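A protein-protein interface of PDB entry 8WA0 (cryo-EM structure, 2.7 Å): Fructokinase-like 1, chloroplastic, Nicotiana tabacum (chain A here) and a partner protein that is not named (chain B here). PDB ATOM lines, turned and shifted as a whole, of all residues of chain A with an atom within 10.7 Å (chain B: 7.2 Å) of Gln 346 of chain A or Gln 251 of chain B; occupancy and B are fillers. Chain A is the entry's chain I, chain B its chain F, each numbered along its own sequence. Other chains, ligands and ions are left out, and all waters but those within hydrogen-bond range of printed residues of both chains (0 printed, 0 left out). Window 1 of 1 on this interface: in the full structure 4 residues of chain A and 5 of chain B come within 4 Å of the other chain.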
ATOM      1  N   ARG A 339     -12.084  18.349 -16.183  1.00  0.00           N
ATOM      2  CA  ARG A 339     -12.697  17.378 -15.286  1.00  0.00           C
ATOM      3  C   ARG A 339     -12.180  17.562 -13.875  1.00  0.00           C
ATOM      4  O   ARG A 339     -12.936  17.441 -12.912  1.00  0.00           O
ATOM      5  CB  ARG A 339     -12.418  15.957 -15.766  1.00  0.00           C
ATOM      6  CG  ARG A 339     -13.406  15.446 -16.801  1.00  0.00           C
ATOM      7  CD  ARG A 339     -12.689  14.812 -17.981  1.00  0.00           C
ATOM      8  NE  ARG A 339     -11.572  13.975 -17.558  1.00  0.00           N
ATOM      9  CZ  ARG A 339     -10.738  13.368 -18.395  1.00  0.00           C
ATOM     10  NH1 ARG A 339     -10.893  13.509 -19.704  1.00  0.00           N
ATOM     11  NH2 ARG A 339      -9.747  12.624 -17.924  1.00  0.00           N
ATOM     12  N   LYS A 340     -10.892  17.858 -13.745  1.00  0.00           N
ATOM     13  CA  LYS A 340     -10.313  18.050 -12.447  1.00  0.00           C
ATOM     14  C   LYS A 340     -10.936  19.197 -11.703  1.00  0.00           C
ATOM     15  O   LYS A 340     -11.175  19.096 -10.518  1.00  0.00           O
ATOM     16  CB  LYS A 340      -8.832  18.325 -12.582  1.00  0.00           C
ATOM     17  CG  LYS A 340      -7.965  17.102 -12.795  1.00  0.00           C
ATOM     18  CD  LYS A 340      -6.543  17.525 -13.121  1.00  0.00           C
ATOM     19  CE  LYS A 340      -6.037  18.586 -12.158  1.00  0.00           C
ATOM     20  NZ  LYS A 340      -5.869  18.065 -10.775  1.00  0.00           N
ATOM     21  N   ASN A 342     -13.846  20.325 -11.737  1.00  0.00           N
ATOM     22  CA  ASN A 342     -15.183  20.042 -11.264  1.00  0.00           C
ATOM     23  C   ASN A 342     -15.286  18.879 -10.286  1.00  0.00           C
ATOM     24  O   ASN A 342     -16.355  18.314 -10.136  1.00  0.00           O
ATOM     25  CB  ASN A 342     -16.079  19.777 -12.452  1.00  0.00           C
ATOM     26  CG  ASN A 342     -16.080  20.919 -13.438  1.00  0.00           C
ATOM     27  OD1 ASN A 342     -15.844  22.066 -13.073  1.00  0.00           O
ATOM     28  ND2 ASN A 342     -16.354  20.611 -14.696  1.00  0.00           N
ATOM     29  N   TYR A 343     -14.202  18.504  -9.627  1.00  0.00           N
ATOM     30  CA  TYR A 343     -14.231  17.457  -8.621  1.00  0.00           C
ATOM     31  C   TYR A 343     -14.563  18.025  -7.311  1.00  0.00           C
ATOM     32  O   TYR A 343     -13.824  18.838  -6.798  1.00  0.00           O
ATOM     33  CB  TYR A 343     -12.877  16.830  -8.480  1.00  0.00           C
ATOM     34  CG  TYR A 343     -12.772  15.682  -7.512  1.00  0.00           C
ATOM     35  CD1 TYR A 343     -13.157  14.410  -7.879  1.00  0.00           C
ATOM     36  CD2 TYR A 343     -12.248  15.863  -6.248  1.00  0.00           C
ATOM     37  CE1 TYR A 343     -13.050  13.354  -7.005  1.00  0.00           C
ATOM     38  CE2 TYR A 343     -12.144  14.815  -5.365  1.00  0.00           C
ATOM     39  CZ  TYR A 343     -12.545  13.563  -5.751  1.00  0.00           C
ATOM     40  OH  TYR A 343     -12.438  12.513  -4.872  1.00  0.00           O
ATOM     41  N   ARG A 344     -15.667  17.613  -6.746  1.00  0.00           N
ATOM     42  CA  ARG A 344     -16.072  18.067  -5.465  1.00  0.00           C
ATOM     43  C   ARG A 344     -16.163  16.823  -4.658  1.00  0.00           C
ATOM     44  O   ARG A 344     -16.778  15.879  -5.091  1.00  0.00           O
ATOM     45  CB  ARG A 344     -17.393  18.759  -5.605  1.00  0.00           C
ATOM     46  CG  ARG A 344     -17.284  20.090  -6.320  1.00  0.00           C
ATOM     47  CD  ARG A 344     -18.638  20.693  -6.626  1.00  0.00           C
ATOM     48  NE  ARG A 344     -18.503  21.948  -7.359  1.00  0.00           N
ATOM     49  CZ  ARG A 344     -19.528  22.679  -7.781  1.00  0.00           C
ATOM     50  NH1 ARG A 344     -20.771  22.281  -7.543  1.00  0.00           N
ATOM     51  NH2 ARG A 344     -19.313  23.809  -8.441  1.00  0.00           N
ATOM     52  N   PRO A 345     -15.537  16.784  -3.497  1.00  0.00           N
ATOM     53  CA  PRO A 345     -15.479  15.571  -2.706  1.00  0.00           C
ATOM     54  C   PRO A 345     -16.788  15.103  -2.057  1.00  0.00           C
ATOM     55  O   PRO A 345     -17.502  15.955  -1.562  1.00  0.00           O
ATOM     56  CB  PRO A 345     -14.449  15.952  -1.685  1.00  0.00           C
ATOM     57  N   GLN A 346     -17.115  13.817  -2.051  1.00  0.00           N
ATOM     58  CA  GLN A 346     -18.401  13.292  -1.530  1.00  0.00           C
ATOM     59  C   GLN A 346     -18.779  13.294  -0.093  1.00  0.00           C
ATOM     60  O   GLN A 346     -19.898  13.634   0.240  1.00  0.00           O
ATOM     61  CB  GLN A 346     -18.625  11.878  -2.032  1.00  0.00           C
ATOM     62  CG  GLN A 346     -20.065  11.466  -2.217  1.00  0.00           C
ATOM     63  CD  GLN A 346     -20.179  10.057  -2.742  1.00  0.00           C
ATOM     64  OE1 GLN A 346     -21.273   9.526  -2.898  1.00  0.00           O
ATOM     65  NE2 GLN A 346     -19.046   9.440  -3.013  1.00  0.00           N
ATOM     66  N   TYR A 347     -17.882  12.905   0.785  1.00  0.00           N
ATOM     67  CA  TYR A 347     -18.216  12.801   2.161  1.00  0.00           C
ATOM     68  C   TYR A 347     -17.490  13.797   3.023  1.00  0.00           C
ATOM     69  O   TYR A 347     -18.114  14.551   3.738  1.00  0.00           O
ATOM     70  CB  TYR A 347     -17.906  11.405   2.657  1.00  0.00           C
ATOM     71  CG  TYR A 347     -18.581  10.256   1.966  1.00  0.00           C
ATOM     72  CD1 TYR A 347     -19.896   9.932   2.231  1.00  0.00           C
ATOM     73  CD2 TYR A 347     -17.882   9.461   1.080  1.00  0.00           C
ATOM     74  CE1 TYR A 347     -20.502   8.867   1.606  1.00  0.00           C
ATOM     75  CE2 TYR A 347     -18.483   8.401   0.452  1.00  0.00           C
ATOM     76  CZ  TYR A 347     -19.790   8.109   0.720  1.00  0.00           C
ATOM     77  OH  TYR A 347     -20.376   7.048   0.090  1.00  0.00           O
ATOM     78  N   PHE A 348     -16.173  13.803   2.983  1.00  0.00           N
ATOM     79  CA  PHE A 348     -15.393  14.717   3.790  1.00  0.00           C
ATOM     80  C   PHE A 348     -14.283  15.386   3.030  1.00  0.00           C
ATOM     81  O   PHE A 348     -13.743  14.812   2.107  1.00  0.00           O
ATOM     82  CB  PHE A 348     -14.898  14.072   5.077  1.00  0.00           C
ATOM     83  CG  PHE A 348     -14.265  12.725   4.929  1.00  0.00           C
ATOM     84  CD1 PHE A 348     -13.086  12.553   4.230  1.00  0.00           C
ATOM     85  CD2 PHE A 348     -14.818  11.637   5.570  1.00  0.00           C
ATOM     86  CE1 PHE A 348     -12.501  11.309   4.122  1.00  0.00           C
ATOM     87  CE2 PHE A 348     -14.239  10.392   5.474  1.00  0.00           C
ATOM     88  CZ  PHE A 348     -13.078  10.224   4.749  1.00  0.00           C
ATOM     89  N   ALA A 349     -13.969  16.615   3.371  1.00  0.00           N
ATOM     90  CA  ALA A 349     -12.894  17.327   2.729  1.00  0.00           C
ATOM     91  C   ALA A 349     -11.554  16.931   3.242  1.00  0.00           C
ATOM     92  O   ALA A 349     -11.430  16.543   4.390  1.00  0.00           O
ATOM     93  CB  ALA A 349     -13.091  18.783   2.885  1.00  0.00           C
ATOM     94  N   GLU A 350     -10.534  17.018   2.418  1.00  0.00           N
ATOM     95  CA  GLU A 350      -9.233  16.531   2.798  1.00  0.00           C
ATOM     96  C   GLU A 350      -8.285  17.540   3.311  1.00  0.00           C
ATOM     97  O   GLU A 350      -7.256  17.195   3.837  1.00  0.00           O
ATOM     98  CB  GLU A 350      -8.650  15.836   1.598  1.00  0.00           C
ATOM     99  N   GLN A 354     -10.555  22.954   0.864  1.00  0.00           N
ATOM    100  CA  GLN A 354     -11.688  22.476   0.090  1.00  0.00           C
ATOM    101  C   GLN A 354     -12.992  22.769   0.790  1.00  0.00           C
ATOM    102  O   GLN A 354     -14.046  22.606   0.215  1.00  0.00           O
ATOM    103  CB  GLN A 354     -11.532  21.013  -0.254  1.00  0.00           C
ATOM    104  CG  GLN A 354     -10.122  20.636  -0.655  1.00  0.00           C
ATOM    105  CD  GLN A 354      -9.946  19.144  -0.846  1.00  0.00           C
ATOM    106  OE1 GLN A 354     -10.915  18.413  -1.038  1.00  0.00           O
ATOM    107  NE2 GLN A 354      -8.702  18.684  -0.796  1.00  0.00           N
ATOM    108  N   SER B 246     -17.627  -1.002  -8.962  1.00  0.00           N
ATOM    109  CA  SER B 246     -17.507  -0.116  -7.830  1.00  0.00           C
ATOM    110  C   SER B 246     -17.059   1.229  -8.258  1.00  0.00           C
ATOM    111  O   SER B 246     -17.586   2.220  -7.808  1.00  0.00           O
ATOM    112  CB  SER B 246     -16.492  -0.659  -6.854  1.00  0.00           C
ATOM    113  OG  SER B 246     -16.395   0.165  -5.715  1.00  0.00           O
ATOM    114  N   TYR B 247     -16.096   1.290  -9.146  1.00  0.00           N
ATOM    115  CA  TYR B 247     -15.549   2.559  -9.496  1.00  0.00           C
ATOM    116  C   TYR B 247     -16.583   3.407 -10.131  1.00  0.00           C
ATOM    117  O   TYR B 247     -16.643   4.606  -9.900  1.00  0.00           O
ATOM    118  CB  TYR B 247     -14.337   2.412 -10.367  1.00  0.00           C
ATOM    119  CG  TYR B 247     -13.065   2.111  -9.620  1.00  0.00           C
ATOM    120  CD1 TYR B 247     -12.369   3.109  -8.971  1.00  0.00           C
ATOM    121  CD2 TYR B 247     -12.548   0.833  -9.590  1.00  0.00           C
ATOM    122  CE1 TYR B 247     -11.201   2.834  -8.295  1.00  0.00           C
ATOM    123  CE2 TYR B 247     -11.382   0.550  -8.916  1.00  0.00           C
ATOM    124  CZ  TYR B 247     -10.716   1.555  -8.272  1.00  0.00           C
ATOM    125  OH  TYR B 247      -9.554   1.270  -7.604  1.00  0.00           O
ATOM    126  N   LYS B 248     -17.396   2.810 -10.947  1.00  0.00           N
ATOM    127  CA  LYS B 248     -18.417   3.557 -11.607  1.00  0.00           C
ATOM    128  C   LYS B 248     -19.455   4.119 -10.693  1.00  0.00           C
ATOM    129  O   LYS B 248     -19.871   5.255 -10.849  1.00  0.00           O
ATOM    130  CB  LYS B 248     -19.084   2.689 -12.665  1.00  0.00           C
ATOM    131  N   TYR B 249     -19.902   3.343  -9.735  1.00  0.00           N
ATOM    132  CA  TYR B 249     -20.983   3.808  -8.902  1.00  0.00           C
ATOM    133  C   TYR B 249     -20.569   4.395  -7.561  1.00  0.00           C
ATOM    134  O   TYR B 249     -21.351   5.095  -6.938  1.00  0.00           O
ATOM    135  CB  TYR B 249     -22.024   2.718  -8.689  1.00  0.00           C
ATOM    136  CG  TYR B 249     -22.505   2.027  -9.932  1.00  0.00           C
ATOM    137  CD1 TYR B 249     -23.119   2.733 -10.950  1.00  0.00           C
ATOM    138  CD2 TYR B 249     -22.370   0.659 -10.072  1.00  0.00           C
ATOM    139  CE1 TYR B 249     -23.565   2.095 -12.089  1.00  0.00           C
ATOM    140  CE2 TYR B 249     -22.809   0.009 -11.204  1.00  0.00           C
ATOM    141  CZ  TYR B 249     -23.406   0.732 -12.209  1.00  0.00           C
ATOM    142  OH  TYR B 249     -23.846   0.086 -13.334  1.00  0.00           O
ATOM    143  N   ASP B 250     -19.355   4.140  -7.114  1.00  0.00           N
ATOM    144  CA  ASP B 250     -18.910   4.708  -5.872  1.00  0.00           C
ATOM    145  C   ASP B 250     -17.622   5.476  -6.022  1.00  0.00           C
ATOM    146  O   ASP B 250     -16.575   4.887  -6.199  1.00  0.00           O
ATOM    147  CB  ASP B 250     -18.728   3.594  -4.855  1.00  0.00           C
ATOM    148  CG  ASP B 250     -19.999   2.824  -4.594  1.00  0.00           C
ATOM    149  OD1 ASP B 250     -21.076   3.446  -4.528  1.00  0.00           O
ATOM    150  OD2 ASP B 250     -19.917   1.589  -4.434  1.00  0.00           O
ATOM    151  N   GLN B 251     -17.691   6.794  -5.948  1.00  0.00           N
ATOM    152  CA  GLN B 251     -16.522   7.625  -6.097  1.00  0.00           C
ATOM    153  C   GLN B 251     -15.464   7.593  -5.024  1.00  0.00           C
ATOM    154  O   GLN B 251     -14.297   7.427  -5.332  1.00  0.00           O
ATOM    155  CB  GLN B 251     -16.981   9.051  -6.326  1.00  0.00           C
ATOM    156  CG  GLN B 251     -15.923  10.130  -6.280  1.00  0.00           C
ATOM    157  CD  GLN B 251     -16.535  11.512  -6.270  1.00  0.00           C
ATOM    158  OE1 GLN B 251     -16.008  12.431  -5.657  1.00  0.00           O
ATOM    159  NE2 GLN B 251     -17.666  11.659  -6.937  1.00  0.00           N
ATOM    160  N   ASP B 252     -15.848   7.682  -3.769  1.00  0.00           N
ATOM    161  CA  ASP B 252     -14.880   7.736  -2.708  1.00  0.00           C
ATOM    162  C   ASP B 252     -15.166   6.707  -1.651  1.00  0.00           C
ATOM    163  O   ASP B 252     -16.320   6.497  -1.310  1.00  0.00           O
ATOM    164  CB  ASP B 252     -14.932   9.098  -2.087  1.00  0.00           C
ATOM    165  CG  ASP B 252     -14.395  10.182  -2.991  1.00  0.00           C
ATOM    166  OD1 ASP B 252     -13.414   9.929  -3.723  1.00  0.00           O
ATOM    167  OD2 ASP B 252     -14.942  11.303  -2.952  1.00  0.00           O
ATOM    168  N   TYR B 253     -14.151   6.060  -1.119  1.00  0.00           N
ATOM    169  CA  TYR B 253     -14.341   5.061  -0.101  1.00  0.00           C
ATOM    170  C   TYR B 253     -14.748   5.608   1.227  1.00  0.00           C
ATOM    171  O   TYR B 253     -14.220   6.611   1.662  1.00  0.00           O
ATOM    172  CB  TYR B 253     -13.062   4.274   0.032  1.00  0.00           C
ATOM    173  CG  TYR B 253     -13.002   3.234   1.108  1.00  0.00           C
ATOM    174  CD1 TYR B 253     -13.606   2.013   0.946  1.00  0.00           C
ATOM    175  CD2 TYR B 253     -12.292   3.462   2.270  1.00  0.00           C
ATOM    176  CE1 TYR B 253     -13.539   1.056   1.929  1.00  0.00           C
ATOM    177  CE2 TYR B 253     -12.219   2.507   3.255  1.00  0.00           C
ATOM    178  CZ  TYR B 253     -12.850   1.308   3.074  1.00  0.00           C
ATOM    179  OH  TYR B 253     -12.779   0.351   4.047  1.00  0.00           O
ATOM    180  N   ARG B 260     -10.644  -1.349  -2.637  1.00  0.00           N
ATOM    181  CA  ARG B 260     -10.145  -1.465  -3.950  1.00  0.00           C
ATOM    182  C   ARG B 260      -8.751  -0.936  -3.956  1.00  0.00           C
ATOM    183  O   ARG B 260      -8.317  -0.314  -2.998  1.00  0.00           O
ATOM    184  CB  ARG B 260     -11.016  -0.622  -4.835  1.00  0.00           C
ATOM    185  CG  ARG B 260     -11.451   0.683  -4.215  1.00  0.00           C
ATOM    186  CD  ARG B 260     -12.706   1.176  -4.894  1.00  0.00           C
ATOM    187  NE  ARG B 260     -12.907   2.597  -4.682  1.00  0.00           N
ATOM    188  CZ  ARG B 260     -13.903   3.282  -5.218  1.00  0.00           C
ATOM    189  NH1 ARG B 260     -14.783   2.667  -5.988  1.00  0.00           N
ATOM    190  NH2 ARG B 260     -14.017   4.575  -4.987  1.00  0.00           N
ATOM    191  N   PHE B 365     -28.953   4.626  -0.206  1.00  0.00           N
ATOM    192  CA  PHE B 365     -28.380   5.626  -1.074  1.00  0.00           C
ATOM    193  C   PHE B 365     -29.424   6.074  -2.049  1.00  0.00           C
ATOM    194  O   PHE B 365     -29.966   5.258  -2.755  1.00  0.00           O
ATOM    195  CB  PHE B 365     -27.286   5.033  -1.916  1.00  0.00           C
ATOM    196  CG  PHE B 365     -25.939   4.991  -1.308  1.00  0.00           C
ATOM    197  CD1 PHE B 365     -25.282   6.140  -0.958  1.00  0.00           C
ATOM    198  CD2 PHE B 365     -25.285   3.797  -1.209  1.00  0.00           C
ATOM    199  CE1 PHE B 365     -24.012   6.088  -0.437  1.00  0.00           C
ATOM    200  CE2 PHE B 365     -24.024   3.729  -0.694  1.00  0.00           C
ATOM    201  CZ  PHE B 365     -23.382   4.877  -0.306  1.00  0.00           C
ATOM    202  N   ARG B 367     -29.697   7.274  -5.194  1.00  0.00           N
ATOM    203  CA  ARG B 367     -28.761   7.427  -6.281  1.00  0.00           C
ATOM    204  C   ARG B 367     -29.214   8.272  -7.384  1.00  0.00           C
ATOM    205  O   ARG B 367     -30.361   8.685  -7.418  1.00  0.00           O
ATOM    206  CB  ARG B 367     -28.295   6.070  -6.779  1.00  0.00           C
ATOM    207  CG  ARG B 367     -28.562   4.917  -5.859  1.00  0.00           C
ATOM    208  CD  ARG B 367     -27.306   4.362  -5.232  1.00  0.00           C
ATOM    209  NE  ARG B 367     -26.127   4.572  -6.041  1.00  0.00           N
ATOM    210  CZ  ARG B 367     -24.970   3.973  -5.815  1.00  0.00           C
ATOM    211  NH1 ARG B 367     -23.941   4.226  -6.593  1.00  0.00           N
ATOM    212  NH2 ARG B 367     -24.845   3.115  -4.824  1.00  0.00           N
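Of the 11 printed residues of chain B, 3 touch a printed residue of chain A. Hydrophobic or aromatic side chains of chain B that line the printed part of chain A: Phe 365. Among the printed residues, 7 pairs touch across the chains.
Of the printed residues of chain B, Tyr 343 of chain A touches Gln 251 and Asp 252. Printed residues of chain B within 4 Å of Arg 344 of chain A: Gln 251. Of chain B, only Gln 251 and Asp 252 come within 4 Å of Gln 346 of chain A. Of the printed residues of chain B, Tyr 347 of chain A touches Asp 252 and Phe 365. Lys 248 of chain B touches none of the printed residues of chain A. Of chain A, only Tyr 343 (3.4 Å), Arg 344 (3.6 Å) and Gln 346 (3.9 Å) come within 4 Å of Gln 251 of chain B. Asp 252 of chain B touches just these residues of chain A: Tyr 343 (3.0 Å), Gln 346 (3.4 Å) and Tyr 347 (3.4 Å). Of the printed residues of chain A, Phe 365 of chain B touches Tyr 347. Arg 367 of chain B touches none of the printed residues of chain A. The nearest residue of chain A that does not touch Gln 251 of chain B is Pro 345 of chain A (4.3 Å). The nearest printed residue of chain B that does not touch Tyr 347 of chain A is Tyr 253 of chain B (4.7 Å).
OE1 of Gln 251 of chain B sits close to OD2 of Asp 252 of chain B, 3.1 Å away. The backbone carbonyl oxygen (O) of Gln 251 of chain B is in hydrogen-bond range of the guanidinium group (NH2) of Arg 260 of chain B, 2.9 Å away.
The side-chain carboxylate (OD1) of Asp 252 of chain B lies within hydrogen-bond range of the side-chain hydroxyl (OH) of Tyr 343 of chain A. The backbone NH (N) of Gln 346 of chain A is in hydrogen-bond range of the side-chain carboxylate (OD2) of Asp 252 of chain B, at 3.4 Å.
Among the printed residues, merely in contact across the chains: Tyr 347 of chain A with Asp 252 of chain B, Tyr 343 of chain A with Gln 251 of chain B, Arg 344 of chain A with Gln 251 of chain B, Tyr 347 of chain A with Phe 365 of chain B and Gln 346 of chain A with Gln 251 of chain B.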
